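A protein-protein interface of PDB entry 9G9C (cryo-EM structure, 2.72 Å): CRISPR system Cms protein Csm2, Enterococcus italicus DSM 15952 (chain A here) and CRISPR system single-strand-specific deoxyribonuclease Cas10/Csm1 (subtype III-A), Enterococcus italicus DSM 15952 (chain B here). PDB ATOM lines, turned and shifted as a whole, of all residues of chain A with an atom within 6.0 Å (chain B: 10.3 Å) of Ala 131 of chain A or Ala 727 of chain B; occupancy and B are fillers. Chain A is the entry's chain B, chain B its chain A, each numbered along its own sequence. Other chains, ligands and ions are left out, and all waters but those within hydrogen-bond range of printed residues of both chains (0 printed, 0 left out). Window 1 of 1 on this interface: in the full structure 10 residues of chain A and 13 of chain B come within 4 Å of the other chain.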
ATOM      1  N   LEU A  14       6.337   8.875  12.657  1.00  0.00           N
ATOM      2  CA  LEU A  14       7.091   8.804  11.382  1.00  0.00           C
ATOM      3  C   LEU A  14       6.822  10.099  10.599  1.00  0.00           C
ATOM      4  O   LEU A  14       7.764  10.602   9.956  1.00  0.00           O
ATOM      5  CB  LEU A  14       6.676   7.544  10.628  1.00  0.00           C
ATOM      6  CG  LEU A  14       6.819   6.248  11.434  1.00  0.00           C
ATOM      7  CD1 LEU A  14       6.438   5.022  10.647  1.00  0.00           C
ATOM      8  CD2 LEU A  14       8.231   6.110  11.955  1.00  0.00           C
ATOM      9  N   PHE A 126      13.465   5.725  14.286  1.00  0.00           N
ATOM     10  CA  PHE A 126      14.891   5.968  13.953  1.00  0.00           C
ATOM     11  C   PHE A 126      15.096   5.661  12.478  1.00  0.00           C
ATOM     12  O   PHE A 126      15.798   6.418  11.781  1.00  0.00           O
ATOM     13  CB  PHE A 126      15.801   5.128  14.849  1.00  0.00           C
ATOM     14  CG  PHE A 126      17.191   5.721  15.028  1.00  0.00           C
ATOM     15  CD1 PHE A 126      18.171   5.554  14.057  1.00  0.00           C
ATOM     16  CD2 PHE A 126      17.518   6.430  16.176  1.00  0.00           C
ATOM     17  CE1 PHE A 126      19.433   6.099  14.223  1.00  0.00           C
ATOM     18  CE2 PHE A 126      18.784   6.967  16.341  1.00  0.00           C
ATOM     19  CZ  PHE A 126      19.737   6.802  15.364  1.00  0.00           C
ATOM     20  N   GLU A 127      14.484   4.574  12.005  1.00  0.00           N
ATOM     21  CA  GLU A 127      14.611   4.184  10.579  1.00  0.00           C
ATOM     22  C   GLU A 127      13.994   5.275   9.692  1.00  0.00           C
ATOM     23  O   GLU A 127      14.590   5.592   8.645  1.00  0.00           O
ATOM     24  CB  GLU A 127      13.935   2.829  10.385  1.00  0.00           C
ATOM     25  CG  GLU A 127      13.924   2.353   8.937  1.00  0.00           C
ATOM     26  CD  GLU A 127      13.071   1.116   8.738  1.00  0.00           C
ATOM     27  OE1 GLU A 127      12.469   0.641   9.723  1.00  0.00           O
ATOM     28  OE2 GLU A 127      13.014   0.626   7.595  1.00  0.00           O
ATOM     29  N   ALA A 128      12.847   5.828  10.104  1.00  0.00           N
ATOM     30  CA  ALA A 128      12.212   6.916   9.324  1.00  0.00           C
ATOM     31  C   ALA A 128      13.133   8.134   9.288  1.00  0.00           C
ATOM     32  O   ALA A 128      13.307   8.723   8.209  1.00  0.00           O
ATOM     33  CB  ALA A 128      10.880   7.268   9.934  1.00  0.00           C
ATOM     34  N   LEU A 129      13.756   8.459  10.422  1.00  0.00           N
ATOM     35  CA  LEU A 129      14.722   9.582  10.446  1.00  0.00           C
ATOM     36  C   LEU A 129      15.763   9.318   9.358  1.00  0.00           C
ATOM     37  O   LEU A 129      16.099  10.261   8.617  1.00  0.00           O
ATOM     38  CB  LEU A 129      15.385   9.697  11.815  1.00  0.00           C
ATOM     39  CG  LEU A 129      14.471  10.062  12.984  1.00  0.00           C
ATOM     40  CD1 LEU A 129      15.262   9.895  14.264  1.00  0.00           C
ATOM     41  CD2 LEU A 129      14.012  11.495  12.825  1.00  0.00           C
ATOM     42  N   VAL A 130      16.254   8.076   9.278  1.00  0.00           N
ATOM     43  CA  VAL A 130      17.290   7.789   8.286  1.00  0.00           C
ATOM     44  C   VAL A 130      16.722   7.875   6.872  1.00  0.00           C
ATOM     45  O   VAL A 130      17.340   8.455   5.968  1.00  0.00           O
ATOM     46  CB  VAL A 130      17.920   6.410   8.560  1.00  0.00           C
ATOM     47  CG1 VAL A 130      18.956   6.079   7.501  1.00  0.00           C
ATOM     48  CG2 VAL A 130      18.539   6.378   9.946  1.00  0.00           C
ATOM     49  N   ALA A 131      15.534   7.304   6.663  1.00  0.00           N
ATOM     50  CA  ALA A 131      14.927   7.277   5.335  1.00  0.00           C
ATOM     51  C   ALA A 131      14.604   8.679   4.839  1.00  0.00           C
ATOM     52  O   ALA A 131      14.820   8.994   3.665  1.00  0.00           O
ATOM     53  CB  ALA A 131      13.665   6.419   5.357  1.00  0.00           C
ATOM     54  N   TYR A 132      14.080   9.521   5.733  1.00  0.00           N
ATOM     55  CA  TYR A 132      13.723  10.914   5.350  1.00  0.00           C
ATOM     56  C   TYR A 132      15.001  11.718   5.125  1.00  0.00           C
ATOM     57  O   TYR A 132      15.034  12.542   4.193  1.00  0.00           O
ATOM     58  CB  TYR A 132      12.776  11.445   6.427  1.00  0.00           C
ATOM     59  CG  TYR A 132      11.388  10.832   6.307  1.00  0.00           C
ATOM     60  CD1 TYR A 132      10.775  10.701   5.069  1.00  0.00           C
ATOM     61  CD2 TYR A 132      10.719  10.337   7.419  1.00  0.00           C
ATOM     62  CE1 TYR A 132       9.518  10.133   4.944  1.00  0.00           C
ATOM     63  CE2 TYR A 132       9.464   9.765   7.307  1.00  0.00           C
ATOM     64  CZ  TYR A 132       8.862   9.664   6.067  1.00  0.00           C
ATOM     65  OH  TYR A 132       7.625   9.100   5.952  1.00  0.00           O
ATOM     66  N   ALA A 133      16.031  11.484   5.941  1.00  0.00           N
ATOM     67  CA  ALA A 133      17.298  12.163   5.709  1.00  0.00           C
ATOM     68  C   ALA A 133      17.846  11.828   4.330  1.00  0.00           C
ATOM     69  O   ALA A 133      18.361  12.704   3.627  1.00  0.00           O
ATOM     70  CB  ALA A 133      18.303  11.787   6.796  1.00  0.00           C
ATOM     71  N   LYS A 134      17.661  10.583   3.899  1.00  0.00           N
ATOM     72  CA  LYS A 134      18.104  10.186   2.540  1.00  0.00           C
ATOM     73  C   LYS A 134      17.215  10.883   1.504  1.00  0.00           C
ATOM     74  O   LYS A 134      17.764  11.429   0.525  1.00  0.00           O
ATOM     75  CB  LYS A 134      17.988   8.667   2.399  1.00  0.00           C
ATOM     76  CG  LYS A 134      18.429   8.082   1.068  1.00  0.00           C
ATOM     77  CD  LYS A 134      19.923   8.242   0.819  1.00  0.00           C
ATOM     78  CE  LYS A 134      20.364   7.530  -0.418  1.00  0.00           C
ATOM     79  NZ  LYS A 134      19.649   8.018  -1.598  1.00  0.00           N
ATOM     80  N   PHE A 135      15.899  10.872   1.723  1.00  0.00           N
ATOM     81  CA  PHE A 135      14.949  11.452   0.736  1.00  0.00           C
ATOM     82  C   PHE A 135      15.207  12.943   0.556  1.00  0.00           C
ATOM     83  O   PHE A 135      15.152  13.416  -0.595  1.00  0.00           O
ATOM     84  CB  PHE A 135      13.522  11.164   1.213  1.00  0.00           C
ATOM     85  CG  PHE A 135      12.426  11.520   0.219  1.00  0.00           C
ATOM     86  CD1 PHE A 135      12.157  10.695  -0.868  1.00  0.00           C
ATOM     87  CD2 PHE A 135      11.646  12.656   0.389  1.00  0.00           C
ATOM     88  CE1 PHE A 135      11.153  11.011  -1.769  1.00  0.00           C
ATOM     89  CE2 PHE A 135      10.644  12.968  -0.516  1.00  0.00           C
ATOM     90  CZ  PHE A 135      10.399  12.146  -1.591  1.00  0.00           C
ATOM     91  N   TYR A 136      15.491  13.666   1.641  1.00  0.00           N
ATOM     92  CA  TYR A 136      15.622  15.147   1.513  1.00  0.00           C
ATOM     93  C   TYR A 136      17.045  15.589   1.177  1.00  0.00           C
ATOM     94  O   TYR A 136      17.269  16.809   1.105  1.00  0.00           O
ATOM     95  CB  TYR A 136      15.136  15.768   2.825  1.00  0.00           C
ATOM     96  CG  TYR A 136      13.622  15.763   2.980  1.00  0.00           C
ATOM     97  CD1 TYR A 136      12.795  15.925   1.876  1.00  0.00           C
ATOM     98  CD2 TYR A 136      13.022  15.584   4.219  1.00  0.00           C
ATOM     99  CE1 TYR A 136      11.418  15.922   2.004  1.00  0.00           C
ATOM    100  CE2 TYR A 136      11.645  15.576   4.361  1.00  0.00           C
ATOM    101  CZ  TYR A 136      10.842  15.744   3.248  1.00  0.00           C
ATOM    102  OH  TYR A 136       9.484  15.742   3.364  1.00  0.00           O
ATOM    103  N   LEU B 717       5.686  -2.445  -0.645  1.00  0.00           N
ATOM    104  CA  LEU B 717       5.538  -1.372   0.367  1.00  0.00           C
ATOM    105  C   LEU B 717       4.101  -0.845   0.327  1.00  0.00           C
ATOM    106  O   LEU B 717       3.492  -0.705   1.407  1.00  0.00           O
ATOM    107  CB  LEU B 717       6.544  -0.276   0.029  1.00  0.00           C
ATOM    108  CG  LEU B 717       8.016  -0.695   0.040  1.00  0.00           C
ATOM    109  CD1 LEU B 717       8.834   0.199  -0.869  1.00  0.00           C
ATOM    110  CD2 LEU B 717       8.547  -0.629   1.456  1.00  0.00           C
ATOM    111  N   LEU B 718       3.576  -0.585  -0.874  1.00  0.00           N
ATOM    112  CA  LEU B 718       2.221   0.008  -1.003  1.00  0.00           C
ATOM    113  C   LEU B 718       1.189  -0.971  -0.441  1.00  0.00           C
ATOM    114  O   LEU B 718       0.269  -0.526   0.271  1.00  0.00           O
ATOM    115  CB  LEU B 718       1.951   0.306  -2.474  1.00  0.00           C
ATOM    116  CG  LEU B 718       2.893   1.299  -3.160  1.00  0.00           C
ATOM    117  CD1 LEU B 718       2.515   1.416  -4.622  1.00  0.00           C
ATOM    118  CD2 LEU B 718       2.869   2.660  -2.492  1.00  0.00           C
ATOM    119  N   ASN B 720       1.621  -3.376   1.845  1.00  0.00           N
ATOM    120  CA  ASN B 720       1.712  -3.627   3.311  1.00  0.00           C
ATOM    121  C   ASN B 720       0.918  -2.547   4.051  1.00  0.00           C
ATOM    122  O   ASN B 720       0.266  -2.905   5.056  1.00  0.00           O
ATOM    123  CB  ASN B 720       3.164  -3.741   3.756  1.00  0.00           C
ATOM    124  CG  ASN B 720       3.290  -4.357   5.128  1.00  0.00           C
ATOM    125  OD1 ASN B 720       2.789  -5.462   5.361  1.00  0.00           O
ATOM    126  ND2 ASN B 720       3.939  -3.660   6.049  1.00  0.00           N
ATOM    127  N   GLU B 721       1.024  -1.287   3.623  1.00  0.00           N
ATOM    128  CA  GLU B 721       0.195  -0.185   4.193  1.00  0.00           C
ATOM    129  C   GLU B 721       0.693   0.198   5.596  1.00  0.00           C
ATOM    130  O   GLU B 721      -0.037   0.935   6.294  1.00  0.00           O
ATOM    131  CB  GLU B 721      -1.302  -0.512   4.162  1.00  0.00           C
ATOM    132  CG  GLU B 721      -1.900  -0.362   2.767  1.00  0.00           C
ATOM    133  CD  GLU B 721      -2.914  -1.415   2.367  1.00  0.00           C
ATOM    134  OE1 GLU B 721      -3.195  -2.310   3.190  1.00  0.00           O
ATOM    135  OE2 GLU B 721      -3.414  -1.342   1.225  1.00  0.00           O
ATOM    136  N   ASP B 722       1.868  -0.285   6.003  1.00  0.00           N
ATOM    137  CA  ASP B 722       2.444   0.169   7.299  1.00  0.00           C
ATOM    138  C   ASP B 722       2.908   1.618   7.122  1.00  0.00           C
ATOM    139  O   ASP B 722       3.346   1.971   6.005  1.00  0.00           O
ATOM    140  CB  ASP B 722       3.516  -0.775   7.821  1.00  0.00           C
ATOM    141  CG  ASP B 722       3.899  -0.596   9.283  1.00  0.00           C
ATOM    142  OD1 ASP B 722       3.382   0.346   9.919  1.00  0.00           O
ATOM    143  OD2 ASP B 722       4.698  -1.416   9.783  1.00  0.00           O
ATOM    144  N   GLN B 723       2.865   2.410   8.195  1.00  0.00           N
ATOM    145  CA  GLN B 723       3.346   3.813   8.131  1.00  0.00           C
ATOM    146  C   GLN B 723       4.842   3.757   7.783  1.00  0.00           C
ATOM    147  O   GLN B 723       5.305   4.623   7.016  1.00  0.00           O
ATOM    148  CB  GLN B 723       3.036   4.569   9.422  1.00  0.00           C
ATOM    149  CG  GLN B 723       3.176   6.082   9.294  1.00  0.00           C
ATOM    150  CD  GLN B 723       2.656   6.836  10.500  1.00  0.00           C
ATOM    151  OE1 GLN B 723       3.381   7.595  11.153  1.00  0.00           O
ATOM    152  NE2 GLN B 723       1.382   6.636  10.802  1.00  0.00           N
ATOM    153  N   ILE B 724       5.565   2.769   8.319  1.00  0.00           N
ATOM    154  CA  ILE B 724       7.039   2.671   8.096  1.00  0.00           C
ATOM    155  C   ILE B 724       7.287   2.510   6.587  1.00  0.00           C
ATOM    156  O   ILE B 724       8.276   3.078   6.100  1.00  0.00           O
ATOM    157  CB  ILE B 724       7.670   1.542   8.936  1.00  0.00           C
ATOM    158  CG1 ILE B 724       9.187   1.703   9.036  1.00  0.00           C
ATOM    159  CG2 ILE B 724       7.284   0.156   8.419  1.00  0.00           C
ATOM    160  CD1 ILE B 724       9.640   3.105   9.398  1.00  0.00           C
ATOM    161  N   ASN B 725       6.441   1.761   5.879  1.00  0.00           N
ATOM    162  CA  ASN B 725       6.683   1.516   4.432  1.00  0.00           C
ATOM    163  C   ASN B 725       6.645   2.858   3.696  1.00  0.00           C
ATOM    164  O   ASN B 725       7.443   3.027   2.765  1.00  0.00           O
ATOM    165  CB  ASN B 725       5.715   0.493   3.858  1.00  0.00           C
ATOM    166  CG  ASN B 725       5.769  -0.809   4.615  1.00  0.00           C
ATOM    167  OD1 ASN B 725       4.732  -1.315   5.047  1.00  0.00           O
ATOM    168  ND2 ASN B 725       6.958  -1.368   4.772  1.00  0.00           N
ATOM    169  N   ILE B 726       5.732   3.758   4.064  1.00  0.00           N
ATOM    170  CA  ILE B 726       5.745   5.121   3.449  1.00  0.00           C
ATOM    171  C   ILE B 726       7.179   5.663   3.537  1.00  0.00           C
ATOM    172  O   ILE B 726       7.697   6.140   2.504  1.00  0.00           O
ATOM    173  CB  ILE B 726       4.734   6.049   4.145  1.00  0.00           C
ATOM    174  CG1 ILE B 726       3.336   5.435   4.166  1.00  0.00           C
ATOM    175  CG2 ILE B 726       4.731   7.437   3.507  1.00  0.00           C
ATOM    176  CD1 ILE B 726       2.742   5.203   2.788  1.00  0.00           C
ATOM    177  N   ALA B 727       7.798   5.573   4.719  1.00  0.00           N
ATOM    178  CA  ALA B 727       9.192   6.045   4.906  1.00  0.00           C
ATOM    179  C   ALA B 727      10.139   5.177   4.075  1.00  0.00           C
ATOM    180  O   ALA B 727      11.060   5.722   3.440  1.00  0.00           O
ATOM    181  CB  ALA B 727       9.552   6.008   6.370  1.00  0.00           C
ATOM    182  N   ARG B 728       9.916   3.861   4.073  1.00  0.00           N
ATOM    183  CA  ARG B 728      10.809   2.932   3.332  1.00  0.00           C
ATOM    184  C   ARG B 728      10.662   3.171   1.823  1.00  0.00           C
ATOM    185  O   ARG B 728      11.674   3.042   1.107  1.00  0.00           O
ATOM    186  CB  ARG B 728      10.489   1.481   3.705  1.00  0.00           C
ATOM    187  CG  ARG B 728      10.786   1.154   5.160  1.00  0.00           C
ATOM    188  CD  ARG B 728      10.322  -0.236   5.557  1.00  0.00           C
ATOM    189  NE  ARG B 728      10.696  -0.516   6.947  1.00  0.00           N
ATOM    190  CZ  ARG B 728      10.409  -1.623   7.616  1.00  0.00           C
ATOM    191  NH1 ARG B 728       9.782  -2.617   7.018  1.00  0.00           N
ATOM    192  NH2 ARG B 728      10.744  -1.725   8.889  1.00  0.00           N
ATOM    193  N   LEU B 729       9.454   3.504   1.361  1.00  0.00           N
ATOM    194  CA  LEU B 729       9.263   3.828  -0.077  1.00  0.00           C
ATOM    195  C   LEU B 729      10.091   5.072  -0.416  1.00  0.00           C
ATOM    196  O   LEU B 729      10.728   5.084  -1.480  1.00  0.00           O
ATOM    197  CB  LEU B 729       7.788   4.051  -0.405  1.00  0.00           C
ATOM    198  CG  LEU B 729       7.483   4.434  -1.856  1.00  0.00           C
ATOM    199  CD1 LEU B 729       7.651   3.254  -2.794  1.00  0.00           C
ATOM    200  CD2 LEU B 729       6.106   5.050  -1.998  1.00  0.00           C
ATOM    201  N   ALA B 730      10.099   6.062   0.481  1.00  0.00           N
ATOM    202  CA  ALA B 730      10.846   7.313   0.228  1.00  0.00           C
ATOM    203  C   ALA B 730      12.336   6.995   0.109  1.00  0.00           C
ATOM    204  O   ALA B 730      13.007   7.563  -0.774  1.00  0.00           O
ATOM    205  CB  ALA B 730      10.578   8.288   1.345  1.00  0.00           C
ATOM    206  N   TYR B 731      12.838   6.107   0.972  1.00  0.00           N
ATOM    207  CA  TYR B 731      14.263   5.698   0.887  1.00  0.00           C
ATOM    208  C   TYR B 731      14.507   4.997  -0.441  1.00  0.00           C
ATOM    209  O   TYR B 731      15.527   5.276  -1.102  1.00  0.00           O
ATOM    210  CB  TYR B 731      14.528   4.801   2.098  1.00  0.00           C
ATOM    211  CG  TYR B 731      15.984   4.432   2.341  1.00  0.00           C
ATOM    212  CD1 TYR B 731      16.840   5.301   3.003  1.00  0.00           C
ATOM    213  CD2 TYR B 731      16.488   3.198   1.952  1.00  0.00           C
ATOM    214  CE1 TYR B 731      18.163   4.971   3.239  1.00  0.00           C
ATOM    215  CE2 TYR B 731      17.808   2.853   2.187  1.00  0.00           C
ATOM    216  CZ  TYR B 731      18.649   3.743   2.827  1.00  0.00           C
ATOM    217  OH  TYR B 731      19.950   3.411   3.062  1.00  0.00           O
ATOM    218  N   LEU B 732      13.574   4.130  -0.842  1.00  0.00           N
ATOM    219  CA  LEU B 732      13.704   3.420  -2.138  1.00  0.00           C
ATOM    220  C   LEU B 732      13.665   4.440  -3.280  1.00  0.00           C
ATOM    221  O   LEU B 732      14.478   4.310  -4.211  1.00  0.00           O
ATOM    222  CB  LEU B 732      12.571   2.403  -2.263  1.00  0.00           C
ATOM    223  CG  LEU B 732      12.421   1.724  -3.628  1.00  0.00           C
ATOM    224  CD1 LEU B 732      13.562   0.763  -3.905  1.00  0.00           C
ATOM    225  CD2 LEU B 732      11.082   1.023  -3.750  1.00  0.00           C
ATOM    226  N   LEU B 733      12.770   5.425  -3.186  1.00  0.00           N
ATOM    227  CA  LEU B 733      12.636   6.443  -4.257  1.00  0.00           C
ATOM    228  C   LEU B 733      13.933   7.255  -4.376  1.00  0.00           C
ATOM    229  O   LEU B 733      14.364   7.518  -5.517  1.00  0.00           O
ATOM    230  CB  LEU B 733      11.444   7.341  -3.933  1.00  0.00           C
ATOM    231  CG  LEU B 733      10.056   6.750  -4.198  1.00  0.00           C
ATOM    232  CD1 LEU B 733       8.979   7.680  -3.673  1.00  0.00           C
ATOM    233  CD2 LEU B 733       9.861   6.483  -5.679  1.00  0.00           C
ATOM    234  N   ALA B 734      14.528   7.631  -3.240  1.00  0.00           N
ATOM    235  CA  ALA B 734      15.788   8.403  -3.276  1.00  0.00           C
ATOM    236  C   ALA B 734      16.887   7.560  -3.918  1.00  0.00           C
ATOM    237  O   ALA B 734      17.642   8.092  -4.758  1.00  0.00           O
ATOM    238  CB  ALA B 734      16.157   8.797  -1.870  1.00  0.00           C
ATOM    239  N   ARG B 735      16.969   6.283  -3.546  1.00  0.00           N
ATOM    240  CA  ARG B 735      17.941   5.343  -4.164  1.00  0.00           C
ATOM    241  C   ARG B 735      17.595   5.145  -5.648  1.00  0.00           C
ATOM    242  O   ARG B 735      18.535   5.040  -6.459  1.00  0.00           O
ATOM    243  CB  ARG B 735      17.974   4.061  -3.330  1.00  0.00           C
ATOM    244  CG  ARG B 735      18.625   4.317  -1.979  1.00  0.00           C
ATOM    245  CD  ARG B 735      18.830   3.038  -1.195  1.00  0.00           C
ATOM    246  NE  ARG B 735      17.573   2.305  -1.024  1.00  0.00           N
ATOM    247  CZ  ARG B 735      17.378   1.059  -1.426  1.00  0.00           C
ATOM    248  NH1 ARG B 735      18.320   0.437  -2.111  1.00  0.00           N
ATOM    249  NH2 ARG B 735      16.246   0.441  -1.140  1.00  0.00           N
ATOM    250  N   THR B 743       9.079  11.078  -8.666  1.00  0.00           N
ATOM    251  CA  THR B 743       9.440  10.656  -7.295  1.00  0.00           C
ATOM    252  C   THR B 743       8.483  11.299  -6.321  1.00  0.00           C
ATOM    253  O   THR B 743       7.889  10.567  -5.504  1.00  0.00           O
ATOM    254  CB  THR B 743      10.888  11.049  -7.014  1.00  0.00           C
ATOM    255  OG1 THR B 743      11.651  10.405  -8.029  1.00  0.00           O
ATOM    256  CG2 THR B 743      11.361  10.608  -5.642  1.00  0.00           C
ATOM    257  N   ILE B 746       4.805   9.979  -6.915  1.00  0.00           N
ATOM    258  CA  ILE B 746       4.634   8.637  -6.285  1.00  0.00           C
ATOM    259  C   ILE B 746       4.512   8.830  -4.767  1.00  0.00           C
ATOM    260  O   ILE B 746       3.588   8.240  -4.169  1.00  0.00           O
ATOM    261  CB  ILE B 746       5.800   7.704  -6.653  1.00  0.00           C
ATOM    262  CG1 ILE B 746       5.778   7.335  -8.129  1.00  0.00           C
ATOM    263  CG2 ILE B 746       5.805   6.461  -5.765  1.00  0.00           C
ATOM    264  CD1 ILE B 746       6.951   6.477  -8.560  1.00  0.00           C
ATOM    265  N   PHE B 747       5.409   9.620  -4.177  1.00  0.00           N
ATOM    266  CA  PHE B 747       5.391   9.789  -2.702  1.00  0.00           C
ATOM    267  C   PHE B 747       4.025  10.343  -2.291  1.00  0.00           C
ATOM    268  O   PHE B 747       3.398   9.788  -1.368  1.00  0.00           O
ATOM    269  CB  PHE B 747       6.555  10.675  -2.255  1.00  0.00           C
ATOM    270  CG  PHE B 747       6.844  10.570  -0.765  1.00  0.00           C
ATOM    271  CD1 PHE B 747       6.708   9.357  -0.099  1.00  0.00           C
ATOM    272  CD2 PHE B 747       7.220  11.686  -0.026  1.00  0.00           C
ATOM    273  CE1 PHE B 747       6.962   9.263   1.259  1.00  0.00           C
ATOM    274  CE2 PHE B 747       7.474  11.585   1.332  1.00  0.00           C
ATOM    275  CZ  PHE B 747       7.343  10.375   1.970  1.00  0.00           C
ATOM    276  N   SER B 750       1.279   7.732  -2.573  1.00  0.00           N
ATOM    277  CA  SER B 750       1.309   6.696  -1.512  1.00  0.00           C
ATOM    278  C   SER B 750       0.640   7.243  -0.250  1.00  0.00           C
ATOM    279  O   SER B 750      -0.111   6.489   0.401  1.00  0.00           O
ATOM    280  CB  SER B 750       2.718   6.285  -1.222  1.00  0.00           C
ATOM    281  OG  SER B 750       3.458   7.363  -0.668  1.00  0.00           O
ATOM    282  N   GLN B 751       0.871   8.520   0.058  1.00  0.00           N
ATOM    283  CA  GLN B 751       0.333   9.116   1.310  1.00  0.00           C
ATOM    284  C   GLN B 751      -1.197   9.265   1.226  1.00  0.00           C
ATOM    285  O   GLN B 751      -1.857   9.074   2.267  1.00  0.00           O
ATOM    286  CB  GLN B 751       1.107  10.413   1.544  1.00  0.00           C
ATOM    287  CG  GLN B 751       2.589  10.175   1.816  1.00  0.00           C
ATOM    288  CD  GLN B 751       3.437  11.423   1.718  1.00  0.00           C
ATOM    289  OE1 GLN B 751       3.526  12.064   0.665  1.00  0.00           O
ATOM    290  NE2 GLN B 751       4.082  11.775   2.819  1.00  0.00           N
ATOM    291  N   LYS B 756      -3.096   5.924  -3.637  1.00  0.00           N
ATOM    292  CA  LYS B 756      -2.290   4.685  -3.500  1.00  0.00           C
ATOM    293  C   LYS B 756      -3.062   3.525  -4.145  1.00  0.00           C
ATOM    294  O   LYS B 756      -2.423   2.753  -4.881  1.00  0.00           O
ATOM    295  CB  LYS B 756      -1.950   4.365  -2.041  1.00  0.00           C
ATOM    296  CG  LYS B 756      -0.910   3.264  -1.897  1.00  0.00           C
ATOM    297  CD  LYS B 756      -0.321   3.131  -0.500  1.00  0.00           C
ATOM    298  CE  LYS B 756      -1.344   2.787   0.530  1.00  0.00           C
ATOM    299  NZ  LYS B 756      -0.727   2.671   1.852  1.00  0.00           N
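Printed residues of chain B within 4 Å of Leu 14 of chain A: Gln 723 (3.3 Å) and Ile 724 (3.4 Å).
No residue of chain B comes within 4 Å of Val 130 of chain A.
Printed residues of chain B within 4 Å of Tyr 132 of chain A: Ala 727 (3.6 Å) and Phe 747 (3.7 Å).
No residue of chain B comes within 4 Å of Ala 133 of chain A.
Of the printed residues of chain B, Lys 134 of chain A touches Tyr 731 (3.6 Å), Ala 734 (3.6 Å) and Arg 735 (3.7 Å).
Of the printed residues of chain B, Phe 135 of chain A touches Ala 730 (3.2 Å), Ala 734 (3.9 Å), Thr 743 (3.9 Å) and Phe 747 (3.6 Å).
Printed residues of chain A within 4 Å of Ala 727 of chain B: Ala 131 and Tyr 132.
Of the printed residues of chain A, Tyr 731 of chain B touches Ala 131 and Lys 134.
Leu 732 of chain B touches none of the printed residues of chain A.
Printed residues of chain A within 4 Å of Arg 735 of chain B: Lys 134 (3.7 Å).
The nearest residue of chain B that does not touch Ala 131 of chain A is Arg 728 of chain B (4.7 Å).
The nearest printed residue of chain A that does not touch Ala 727 of chain B is Ala 128 of chain A (4.01 Å).
The nearest printed residue of chain A that does not touch Ile 724 of chain B is Ala 128 of chain A (4.3 Å).
O of Phe 747 of chain B sits at hydrogen-bond distance from OG of Ser 750 of chain B.
O of Phe 747 of chain B lies close to OE1 of Gln 751 of chain B, 3.1 Å away.
OE1 of Gln 723 of chain B touches CB of Leu 14 of chain A (3.3 Å).
N of Ile 724 of chain B touches CD1 of Leu 14 of chain A (3.4 Å).
OE1 of Glu 127 of chain A touches CG1 of Ile 724 of chain B (3.5 Å).
Ala 727 of chain B touches Ala 131 of chain A (O to CB, 3.3 Å).
CD1 of Tyr 731 of chain B touches CA of Ala 131 of chain A, 3.6 Å away.
OH of Tyr 132 of chain A touches CA of Ala 727 of chain B (3.6 Å).
CD1 of Tyr 731 of chain B touches CB of Lys 134 of chain A, 3.6 Å away.
Lys 134 of chain A touches Ala 734 of chain B.
O of Ala 730 of chain B touches CD1 of Phe 135 of chain A (3.2 Å).
Phe 135 of chain A touches Thr 743 of chain B (CE1 to CG2, 3.9 Å).
The guanidinium group (NE) of Arg 728 of chain B is in salt-bridge range of the side-chain carboxylate (OE2) of Glu 127 of chain A (2.7 Å).
Printed residues of chain A that touch a printed residue of chain B: Leu 14, Glu 127, Ala 131, Tyr 132, Lys 134 and Phe 135.
Hydrophobic or aromatic side chains of chain B that line the printed part of chain A: Ile 724, Ala 727, Ala 730, Tyr 731, Ala 734 and Phe 747.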
